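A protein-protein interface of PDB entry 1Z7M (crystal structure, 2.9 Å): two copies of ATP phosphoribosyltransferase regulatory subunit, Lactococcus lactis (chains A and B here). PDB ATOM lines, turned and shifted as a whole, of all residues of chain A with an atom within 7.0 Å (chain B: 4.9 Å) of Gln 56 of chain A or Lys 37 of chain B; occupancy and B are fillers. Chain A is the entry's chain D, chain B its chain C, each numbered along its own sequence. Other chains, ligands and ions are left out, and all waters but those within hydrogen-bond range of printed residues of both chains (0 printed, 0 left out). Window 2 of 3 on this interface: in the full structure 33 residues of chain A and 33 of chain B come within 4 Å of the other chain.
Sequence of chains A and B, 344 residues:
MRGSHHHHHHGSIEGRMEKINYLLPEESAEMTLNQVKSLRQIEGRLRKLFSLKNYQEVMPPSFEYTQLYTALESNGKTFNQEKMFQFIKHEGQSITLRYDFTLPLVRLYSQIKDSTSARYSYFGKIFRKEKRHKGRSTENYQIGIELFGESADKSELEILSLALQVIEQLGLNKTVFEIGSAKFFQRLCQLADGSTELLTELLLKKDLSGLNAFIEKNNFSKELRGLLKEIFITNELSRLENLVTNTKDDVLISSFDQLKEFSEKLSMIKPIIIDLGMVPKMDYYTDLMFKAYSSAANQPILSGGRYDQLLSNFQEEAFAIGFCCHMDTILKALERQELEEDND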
ATOM      1  N   PHE A  50     -28.380 -24.250   3.414  1.00  0.00           N
ATOM      2  CA  PHE A  50     -28.295 -24.154   4.874  1.00  0.00           C
ATOM      3  C   PHE A  50     -26.984 -23.576   5.378  1.00  0.00           C
ATOM      4  O   PHE A  50     -26.985 -22.685   6.220  1.00  0.00           O
ATOM      5  CB  PHE A  50     -28.506 -25.527   5.527  1.00  0.00           C
ATOM      6  CG  PHE A  50     -29.883 -26.089   5.339  1.00  0.00           C
ATOM      7  CD1 PHE A  50     -30.126 -27.435   5.579  1.00  0.00           C
ATOM      8  CD2 PHE A  50     -30.932 -25.284   4.898  1.00  0.00           C
ATOM      9  CE1 PHE A  50     -31.383 -27.975   5.381  1.00  0.00           C
ATOM     10  CE2 PHE A  50     -32.198 -25.819   4.696  1.00  0.00           C
ATOM     11  CZ  PHE A  50     -32.423 -27.168   4.937  1.00  0.00           C
ATOM     12  N   SER A  51     -25.870 -24.095   4.873  1.00  0.00           N
ATOM     13  CA  SER A  51     -24.556 -23.630   5.307  1.00  0.00           C
ATOM     14  C   SER A  51     -24.298 -22.194   4.864  1.00  0.00           C
ATOM     15  O   SER A  51     -23.505 -21.479   5.482  1.00  0.00           O
ATOM     16  CB  SER A  51     -23.456 -24.566   4.784  1.00  0.00           C
ATOM     17  OG  SER A  51     -23.658 -24.899   3.428  1.00  0.00           O
ATOM     18  N   LYS A  53     -26.446 -20.061   5.063  1.00  0.00           N
ATOM     19  CA  LYS A  53     -27.200 -19.287   6.039  1.00  0.00           C
ATOM     20  C   LYS A  53     -26.661 -19.583   7.423  1.00  0.00           C
ATOM     21  O   LYS A  53     -27.279 -19.264   8.436  1.00  0.00           O
ATOM     22  CB  LYS A  53     -28.673 -19.632   5.955  1.00  0.00           C
ATOM     23  CG  LYS A  53     -29.237 -19.418   4.565  1.00  0.00           C
ATOM     24  CD  LYS A  53     -29.251 -17.959   4.174  1.00  0.00           C
ATOM     25  CE  LYS A  53     -29.984 -17.769   2.858  1.00  0.00           C
ATOM     26  NZ  LYS A  53     -30.409 -16.350   2.675  1.00  0.00           N
ATOM     27  N   ASN A  54     -25.496 -20.221   7.438  1.00  0.00           N
ATOM     28  CA  ASN A  54     -24.790 -20.543   8.664  1.00  0.00           C
ATOM     29  C   ASN A  54     -25.474 -21.553   9.597  1.00  0.00           C
ATOM     30  O   ASN A  54     -25.478 -21.374  10.815  1.00  0.00           O
ATOM     31  CB  ASN A  54     -24.511 -19.237   9.404  1.00  0.00           C
ATOM     32  CG  ASN A  54     -23.288 -19.315  10.281  1.00  0.00           C
ATOM     33  OD1 ASN A  54     -22.202 -19.690   9.829  1.00  0.00           O
ATOM     34  ND2 ASN A  54     -23.449 -18.952  11.545  1.00  0.00           N
ATOM     35  N   TYR A  55     -26.041 -22.617   9.026  1.00  0.00           N
ATOM     36  CA  TYR A  55     -26.711 -23.656   9.810  1.00  0.00           C
ATOM     37  C   TYR A  55     -25.800 -24.858   9.918  1.00  0.00           C
ATOM     38  O   TYR A  55     -25.495 -25.513   8.920  1.00  0.00           O
ATOM     39  CB  TYR A  55     -28.021 -24.077   9.155  1.00  0.00           C
ATOM     40  CG  TYR A  55     -29.192 -23.208   9.527  1.00  0.00           C
ATOM     41  CD1 TYR A  55     -29.338 -21.929   8.991  1.00  0.00           C
ATOM     42  CD2 TYR A  55     -30.147 -23.657  10.438  1.00  0.00           C
ATOM     43  CE1 TYR A  55     -30.408 -21.115   9.353  1.00  0.00           C
ATOM     44  CE2 TYR A  55     -31.220 -22.857  10.810  1.00  0.00           C
ATOM     45  CZ  TYR A  55     -31.347 -21.586  10.263  1.00  0.00           C
ATOM     46  OH  TYR A  55     -32.419 -20.795  10.618  1.00  0.00           O
ATOM     47  N   GLN A  56     -25.374 -25.140  11.143  1.00  0.00           N
ATOM     48  CA  GLN A  56     -24.469 -26.243  11.407  1.00  0.00           C
ATOM     49  C   GLN A  56     -25.214 -27.548  11.460  1.00  0.00           C
ATOM     50  O   GLN A  56     -26.227 -27.653  12.136  1.00  0.00           O
ATOM     51  CB  GLN A  56     -23.741 -26.023  12.737  1.00  0.00           C
ATOM     52  CG  GLN A  56     -23.046 -24.682  12.837  1.00  0.00           C
ATOM     53  CD  GLN A  56     -22.434 -24.266  11.512  1.00  0.00           C
ATOM     54  OE1 GLN A  56     -21.593 -24.968  10.948  1.00  0.00           O
ATOM     55  NE2 GLN A  56     -22.874 -23.128  10.997  1.00  0.00           N
ATOM     56  N   GLU A  57     -24.721 -28.550  10.751  1.00  0.00           N
ATOM     57  CA  GLU A  57     -25.378 -29.839  10.792  1.00  0.00           C
ATOM     58  C   GLU A  57     -25.024 -30.574  12.082  1.00  0.00           C
ATOM     59  O   GLU A  57     -23.935 -30.401  12.629  1.00  0.00           O
ATOM     60  CB  GLU A  57     -24.964 -30.699   9.597  1.00  0.00           C
ATOM     61  CG  GLU A  57     -25.556 -32.096   9.645  1.00  0.00           C
ATOM     62  CD  GLU A  57     -25.244 -32.931   8.428  1.00  0.00           C
ATOM     63  OE1 GLU A  57     -25.681 -34.096   8.408  1.00  0.00           O
ATOM     64  OE2 GLU A  57     -24.573 -32.438   7.497  1.00  0.00           O
ATOM     65  N   VAL A  58     -25.962 -31.367  12.579  1.00  0.00           N
ATOM     66  CA  VAL A  58     -25.733 -32.175  13.765  1.00  0.00           C
ATOM     67  C   VAL A  58     -26.308 -33.552  13.463  1.00  0.00           C
ATOM     68  O   VAL A  58     -27.256 -33.679  12.684  1.00  0.00           O
ATOM     69  CB  VAL A  58     -26.398 -31.585  15.038  1.00  0.00           C
ATOM     70  CG1 VAL A  58     -27.469 -30.625  14.674  1.00  0.00           C
ATOM     71  CG2 VAL A  58     -26.984 -32.688  15.873  1.00  0.00           C
ATOM     72  N   MET A  59     -25.717 -34.585  14.052  1.00  0.00           N
ATOM     73  CA  MET A  59     -26.179 -35.953  13.841  1.00  0.00           C
ATOM     74  C   MET A  59     -26.509 -36.549  15.194  1.00  0.00           C
ATOM     75  O   MET A  59     -25.641 -37.120  15.852  1.00  0.00           O
ATOM     76  CB  MET A  59     -25.092 -36.772  13.164  1.00  0.00           C
ATOM     77  CG  MET A  59     -24.841 -36.407  11.730  1.00  0.00           C
ATOM     78  SD  MET A  59     -23.329 -37.183  11.140  1.00  0.00           S
ATOM     79  CE  MET A  59     -23.788 -38.913  11.126  1.00  0.00           C
ATOM     80  N   LEU A 105     -31.924 -32.251  19.199  1.00  0.00           N
ATOM     81  CA  LEU A 105     -31.309 -30.969  18.864  1.00  0.00           C
ATOM     82  C   LEU A 105     -31.615 -29.886  19.880  1.00  0.00           C
ATOM     83  O   LEU A 105     -30.853 -28.921  20.041  1.00  0.00           O
ATOM     84  CB  LEU A 105     -31.778 -30.480  17.502  1.00  0.00           C
ATOM     85  CG  LEU A 105     -31.622 -31.430  16.331  1.00  0.00           C
ATOM     86  CD1 LEU A 105     -31.696 -30.618  15.067  1.00  0.00           C
ATOM     87  CD2 LEU A 105     -30.310 -32.158  16.401  1.00  0.00           C
ATOM     88  N   ALA A 118     -28.419 -20.062  17.861  1.00  0.00           N
ATOM     89  CA  ALA A 118     -27.985 -21.394  17.418  1.00  0.00           C
ATOM     90  C   ALA A 118     -28.762 -21.925  16.211  1.00  0.00           C
ATOM     91  O   ALA A 118     -29.986 -22.044  16.267  1.00  0.00           O
ATOM     92  CB  ALA A 118     -28.105 -22.385  18.575  1.00  0.00           C
ATOM     93  N   ARG A 119     -28.050 -22.252  15.132  1.00  0.00           N
ATOM     94  CA  ARG A 119     -28.677 -22.785  13.918  1.00  0.00           C
ATOM     95  C   ARG A 119     -28.252 -24.234  13.632  1.00  0.00           C
ATOM     96  O   ARG A 119     -27.095 -24.502  13.289  1.00  0.00           O
ATOM     97  CB  ARG A 119     -28.339 -21.918  12.696  1.00  0.00           C
ATOM     98  CG  ARG A 119     -28.937 -20.525  12.706  1.00  0.00           C
ATOM     99  CD  ARG A 119     -28.006 -19.504  13.380  1.00  0.00           C
ATOM    100  NE  ARG A 119     -28.701 -18.248  13.677  1.00  0.00           N
ATOM    101  CZ  ARG A 119     -29.279 -17.476  12.761  1.00  0.00           C
ATOM    102  NH1 ARG A 119     -29.238 -17.821  11.480  1.00  0.00           N
ATOM    103  NH2 ARG A 119     -29.937 -16.382  13.132  1.00  0.00           N
ATOM    104  N   TYR A 120     -29.200 -25.161  13.757  1.00  0.00           N
ATOM    105  CA  TYR A 120     -28.943 -26.584  13.525  1.00  0.00           C
ATOM    106  C   TYR A 120     -29.655 -27.150  12.296  1.00  0.00           C
ATOM    107  O   TYR A 120     -30.708 -26.669  11.906  1.00  0.00           O
ATOM    108  CB  TYR A 120     -29.385 -27.375  14.745  1.00  0.00           C
ATOM    109  CG  TYR A 120     -28.613 -27.056  15.991  1.00  0.00           C
ATOM    110  CD1 TYR A 120     -29.190 -27.229  17.249  1.00  0.00           C
ATOM    111  CD2 TYR A 120     -27.288 -26.645  15.927  1.00  0.00           C
ATOM    112  CE1 TYR A 120     -28.464 -27.007  18.420  1.00  0.00           C
ATOM    113  CE2 TYR A 120     -26.551 -26.422  17.084  1.00  0.00           C
ATOM    114  CZ  TYR A 120     -27.141 -26.606  18.329  1.00  0.00           C
ATOM    115  OH  TYR A 120     -26.408 -26.411  19.480  1.00  0.00           O
ATOM    116  N   SER A 121     -29.067 -28.161  11.677  1.00  0.00           N
ATOM    117  CA  SER A 121     -29.692 -28.802  10.537  1.00  0.00           C
ATOM    118  C   SER A 121     -29.459 -30.301  10.693  1.00  0.00           C
ATOM    119  O   SER A 121     -28.546 -30.723  11.398  1.00  0.00           O
ATOM    120  CB  SER A 121     -29.105 -28.291   9.220  1.00  0.00           C
ATOM    121  OG  SER A 121     -27.716 -28.523   9.118  1.00  0.00           O
ATOM    122  N   TYR A 122     -30.292 -31.113  10.063  1.00  0.00           N
ATOM    123  CA  TYR A 122     -30.121 -32.553  10.177  1.00  0.00           C
ATOM    124  C   TYR A 122     -30.588 -33.252   8.911  1.00  0.00           C
ATOM    125  O   TYR A 122     -31.566 -32.849   8.276  1.00  0.00           O
ATOM    126  CB  TYR A 122     -30.879 -33.094  11.406  1.00  0.00           C
ATOM    127  CG  TYR A 122     -32.355 -32.772  11.409  1.00  0.00           C
ATOM    128  CD1 TYR A 122     -33.261 -33.528  10.659  1.00  0.00           C
ATOM    129  CD2 TYR A 122     -32.831 -31.649  12.070  1.00  0.00           C
ATOM    130  CE1 TYR A 122     -34.603 -33.163  10.563  1.00  0.00           C
ATOM    131  CE2 TYR A 122     -34.163 -31.274  11.979  1.00  0.00           C
ATOM    132  CZ  TYR A 122     -35.046 -32.031  11.223  1.00  0.00           C
ATOM    133  OH  TYR A 122     -36.360 -31.625  11.116  1.00  0.00           O
ATOM    134  N   PHE A 123     -29.860 -34.297   8.540  1.00  0.00           N
ATOM    135  CA  PHE A 123     -30.177 -35.095   7.359  1.00  0.00           C
ATOM    136  C   PHE A 123     -30.135 -36.535   7.812  1.00  0.00           C
ATOM    137  O   PHE A 123     -29.075 -37.051   8.155  1.00  0.00           O
ATOM    138  CB  PHE A 123     -29.139 -34.882   6.250  1.00  0.00           C
ATOM    139  CG  PHE A 123     -28.973 -33.449   5.845  1.00  0.00           C
ATOM    140  CD1 PHE A 123     -28.403 -32.527   6.721  1.00  0.00           C
ATOM    141  CD2 PHE A 123     -29.418 -33.012   4.603  1.00  0.00           C
ATOM    142  CE1 PHE A 123     -28.285 -31.190   6.367  1.00  0.00           C
ATOM    143  CE2 PHE A 123     -29.304 -31.677   4.240  1.00  0.00           C
ATOM    144  CZ  PHE A 123     -28.736 -30.762   5.123  1.00  0.00           C
ATOM    145  N   LEU B  33     -20.394 -30.721  16.494  1.00  0.00           N
ATOM    146  CA  LEU B  33     -20.729 -30.066  15.241  1.00  0.00           C
ATOM    147  C   LEU B  33     -19.578 -30.097  14.238  1.00  0.00           C
ATOM    148  O   LEU B  33     -19.807 -30.091  13.028  1.00  0.00           O
ATOM    149  CB  LEU B  33     -21.151 -28.621  15.494  1.00  0.00           C
ATOM    150  CG  LEU B  33     -22.473 -28.391  16.222  1.00  0.00           C
ATOM    151  CD1 LEU B  33     -22.689 -26.893  16.356  1.00  0.00           C
ATOM    152  CD2 LEU B  33     -23.616 -29.044  15.448  1.00  0.00           C
ATOM    153  N   ASN B  34     -18.347 -30.135  14.741  1.00  0.00           N
ATOM    154  CA  ASN B  34     -17.165 -30.153  13.882  1.00  0.00           C
ATOM    155  C   ASN B  34     -16.920 -31.526  13.293  1.00  0.00           C
ATOM    156  O   ASN B  34     -16.541 -31.644  12.131  1.00  0.00           O
ATOM    157  CB  ASN B  34     -15.938 -29.713  14.667  1.00  0.00           C
ATOM    158  CG  ASN B  34     -16.169 -28.415  15.409  1.00  0.00           C
ATOM    159  OD1 ASN B  34     -16.271 -27.340  14.799  1.00  0.00           O
ATOM    160  ND2 ASN B  34     -16.277 -28.505  16.735  1.00  0.00           N
ATOM    161  N   GLN B  35     -17.119 -32.566  14.100  1.00  0.00           N
ATOM    162  CA  GLN B  35     -16.932 -33.927  13.623  1.00  0.00           C
ATOM    163  C   GLN B  35     -17.864 -34.158  12.466  1.00  0.00           C
ATOM    164  O   GLN B  35     -17.468 -34.757  11.472  1.00  0.00           O
ATOM    165  CB  GLN B  35     -17.257 -34.943  14.689  1.00  0.00           C
ATOM    166  CG  GLN B  35     -16.214 -35.096  15.732  1.00  0.00           C
ATOM    167  CD  GLN B  35     -16.669 -36.064  16.785  1.00  0.00           C
ATOM    168  OE1 GLN B  35     -17.609 -35.786  17.535  1.00  0.00           O
ATOM    169  NE2 GLN B  35     -16.026 -37.219  16.842  1.00  0.00           N
ATOM    170  N   VAL B  36     -19.108 -33.706  12.578  1.00  0.00           N
ATOM    171  CA  VAL B  36     -20.017 -33.896  11.469  1.00  0.00           C
ATOM    172  C   VAL B  36     -19.437 -33.202  10.231  1.00  0.00           C
ATOM    173  O   VAL B  36     -19.528 -33.742   9.130  1.00  0.00           O
ATOM    174  CB  VAL B  36     -21.423 -33.377  11.789  1.00  0.00           C
ATOM    175  CG1 VAL B  36     -22.360 -33.650  10.625  1.00  0.00           C
ATOM    176  CG2 VAL B  36     -21.946 -34.075  13.017  1.00  0.00           C
ATOM    177  N   LYS B  37     -18.815 -32.035  10.400  1.00  0.00           N
ATOM    178  CA  LYS B  37     -18.207 -31.349   9.250  1.00  0.00           C
ATOM    179  C   LYS B  37     -17.102 -32.199   8.589  1.00  0.00           C
ATOM    180  O   LYS B  37     -17.062 -32.331   7.372  1.00  0.00           O
ATOM    181  CB  LYS B  37     -17.623 -29.987   9.651  1.00  0.00           C
ATOM    182  CG  LYS B  37     -18.588 -28.834   9.555  1.00  0.00           C
ATOM    183  CD  LYS B  37     -17.855 -27.505   9.383  1.00  0.00           C
ATOM    184  CE  LYS B  37     -18.839 -26.323   9.364  1.00  0.00           C
ATOM    185  NZ  LYS B  37     -19.889 -26.398   8.290  1.00  0.00           N
ATOM    186  N   SER B  38     -16.205 -32.758   9.391  1.00  0.00           N
ATOM    187  CA  SER B  38     -15.137 -33.595   8.864  1.00  0.00           C
ATOM    188  C   SER B  38     -15.751 -34.792   8.149  1.00  0.00           C
ATOM    189  O   SER B  38     -15.402 -35.113   7.007  1.00  0.00           O
ATOM    190  CB  SER B  38     -14.247 -34.127   9.994  1.00  0.00           C
ATOM    191  OG  SER B  38     -13.585 -33.101  10.708  1.00  0.00           O
ATOM    192  N   LEU B  39     -16.657 -35.464   8.848  1.00  0.00           N
ATOM    193  CA  LEU B  39     -17.317 -36.632   8.309  1.00  0.00           C
ATOM    194  C   LEU B  39     -17.923 -36.277   6.954  1.00  0.00           C
ATOM    195  O   LEU B  39     -17.651 -36.942   5.961  1.00  0.00           O
ATOM    196  CB  LEU B  39     -18.385 -37.113   9.293  1.00  0.00           C
ATOM    197  CG  LEU B  39     -19.095 -38.446   9.053  1.00  0.00           C
ATOM    198  CD1 LEU B  39     -20.148 -38.318   7.966  1.00  0.00           C
ATOM    199  CD2 LEU B  39     -18.062 -39.482   8.676  1.00  0.00           C
ATOM    200  N   ARG B  40     -18.710 -35.205   6.905  1.00  0.00           N
ATOM    201  CA  ARG B  40     -19.340 -34.792   5.657  1.00  0.00           C
ATOM    202  C   ARG B  40     -18.343 -34.377   4.575  1.00  0.00           C
ATOM    203  O   ARG B  40     -18.599 -34.589   3.392  1.00  0.00           O
ATOM    204  CB  ARG B  40     -20.348 -33.669   5.906  1.00  0.00           C
ATOM    205  CG  ARG B  40     -21.526 -34.054   6.788  1.00  0.00           C
ATOM    206  CD  ARG B  40     -22.268 -35.282   6.274  1.00  0.00           C
ATOM    207  NE  ARG B  40     -23.366 -35.659   7.166  1.00  0.00           N
ATOM    208  CZ  ARG B  40     -23.830 -36.898   7.299  1.00  0.00           C
ATOM    209  NH1 ARG B  40     -23.283 -37.885   6.593  1.00  0.00           N
ATOM    210  NH2 ARG B  40     -24.837 -37.153   8.131  1.00  0.00           N
ATOM    211  N   GLN B  41     -17.216 -33.782   4.972  1.00  0.00           N
ATOM    212  CA  GLN B  41     -16.166 -33.374   4.024  1.00  0.00           C
ATOM    213  C   GLN B  41     -15.601 -34.609   3.355  1.00  0.00           C
ATOM    214  O   GLN B  41     -15.560 -34.695   2.131  1.00  0.00           O
ATOM    215  CB  GLN B  41     -15.006 -32.695   4.733  1.00  0.00           C
ATOM    216  CG  GLN B  41     -15.140 -31.224   4.890  1.00  0.00           C
ATOM    217  CD  GLN B  41     -14.152 -30.688   5.887  1.00  0.00           C
ATOM    218  OE1 GLN B  41     -14.475 -29.786   6.658  1.00  0.00           O
ATOM    219  NE2 GLN B  41     -12.932 -31.242   5.886  1.00  0.00           N
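Among the printed residues, merely in contact across the chains: Glu 57 of chain A with Leu 33 of chain B, Glu 57 of chain A with Val 36 of chain B, Met 59 of chain A with Val 36 of chain B, Val 58 of chain A with Leu 33 of chain B, Gln 56 of chain A with Leu 33 of chain B and Tyr 120 of chain A with Leu 33 of chain B.
The backbone carbonyl oxygen (O) of Gln 56 of chain A is in hydrogen-bond range of the backbone NH (N) of Ser 121 of chain A (2.9 Å). The backbone NH (N) of Val 58 of chain A is in hydrogen-bond range of the backbone carbonyl oxygen (O) of Ser 121 of chain A, at 2.9 Å. The side-chain hydroxyl (OG) of Ser 121 of chain A sits close to the backbone NH (N) of Glu 57 of chain A (3.4 Å). The backbone carbonyl oxygen (O) of Asn 54 of chain A lies within hydrogen-bond range of the side-chain amide nitrogen (NE2) of Gln 56 of chain A (3.1 Å). The backbone NH (N) of Gln 56 of chain A lies within hydrogen-bond range of the backbone carbonyl oxygen (O) of Arg 119 of chain A (2.8 Å).
Ser 51 of chain A touches none of the printed residues of chain B. Gln 56 of chain A touches just these residues of chain B: Leu 33 (3.9 Å) and Lys 37 (3.5 Å). Printed residues of chain B within 4 Å of Glu 57 of chain A: Leu 33, Val 36 and Arg 40. Printed residues of chain B within 4 Å of Tyr 120 of chain A: Leu 33. Of the printed residues of chain A, Leu 33 of chain B touches Gln 56, Glu 57, Val 58 and Tyr 120. Of the printed residues of chain A, Lys 37 of chain B touches Gln 56 (3.5 Å). The nearest residue of chain A that does not touch Lys 37 of chain B is Ser 51 of chain A (5.3 Å). The nearest printed residue of chain B that does not touch Glu 57 of chain A is Lys 37 of chain B (5.8 Å).
No position is printed for both chains. Of the 9 pairs that touch across the chains among the printed residues, none has its exchanged pair printed and touching as well.
NH2 of Arg 40 of chain B sits at hydrogen-bond distance from SD of Met 59 of chain A (3.4 Å). The guanidinium group (NE) of Arg 40 of chain B is in salt-bridge range of the side-chain carboxylate (OE1) of Glu 57 of chain A, 3.1 Å away. NZ of Lys 37 of chain B lies close to OE1 of Gln 56 of chain A (3.5 Å).
Of the 16 printed residues of chain A, 5 touch a printed residue of chain B. Printed residues of chain A that touch a printed residue of chain B: Gln 56, Glu 57, Val 58, Met 59 and Tyr 120. Hydrophobic or aromatic side chains of chain A within 4 Å of the printed part of chain B: Val 58, Met 59 and Tyr 120. Hydrophobic or aromatic side chains of chain B within 4 Å of the printed part of chain A: Leu 33 and Val 36. Among the printed residues, 9 pairs touch across the chains.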
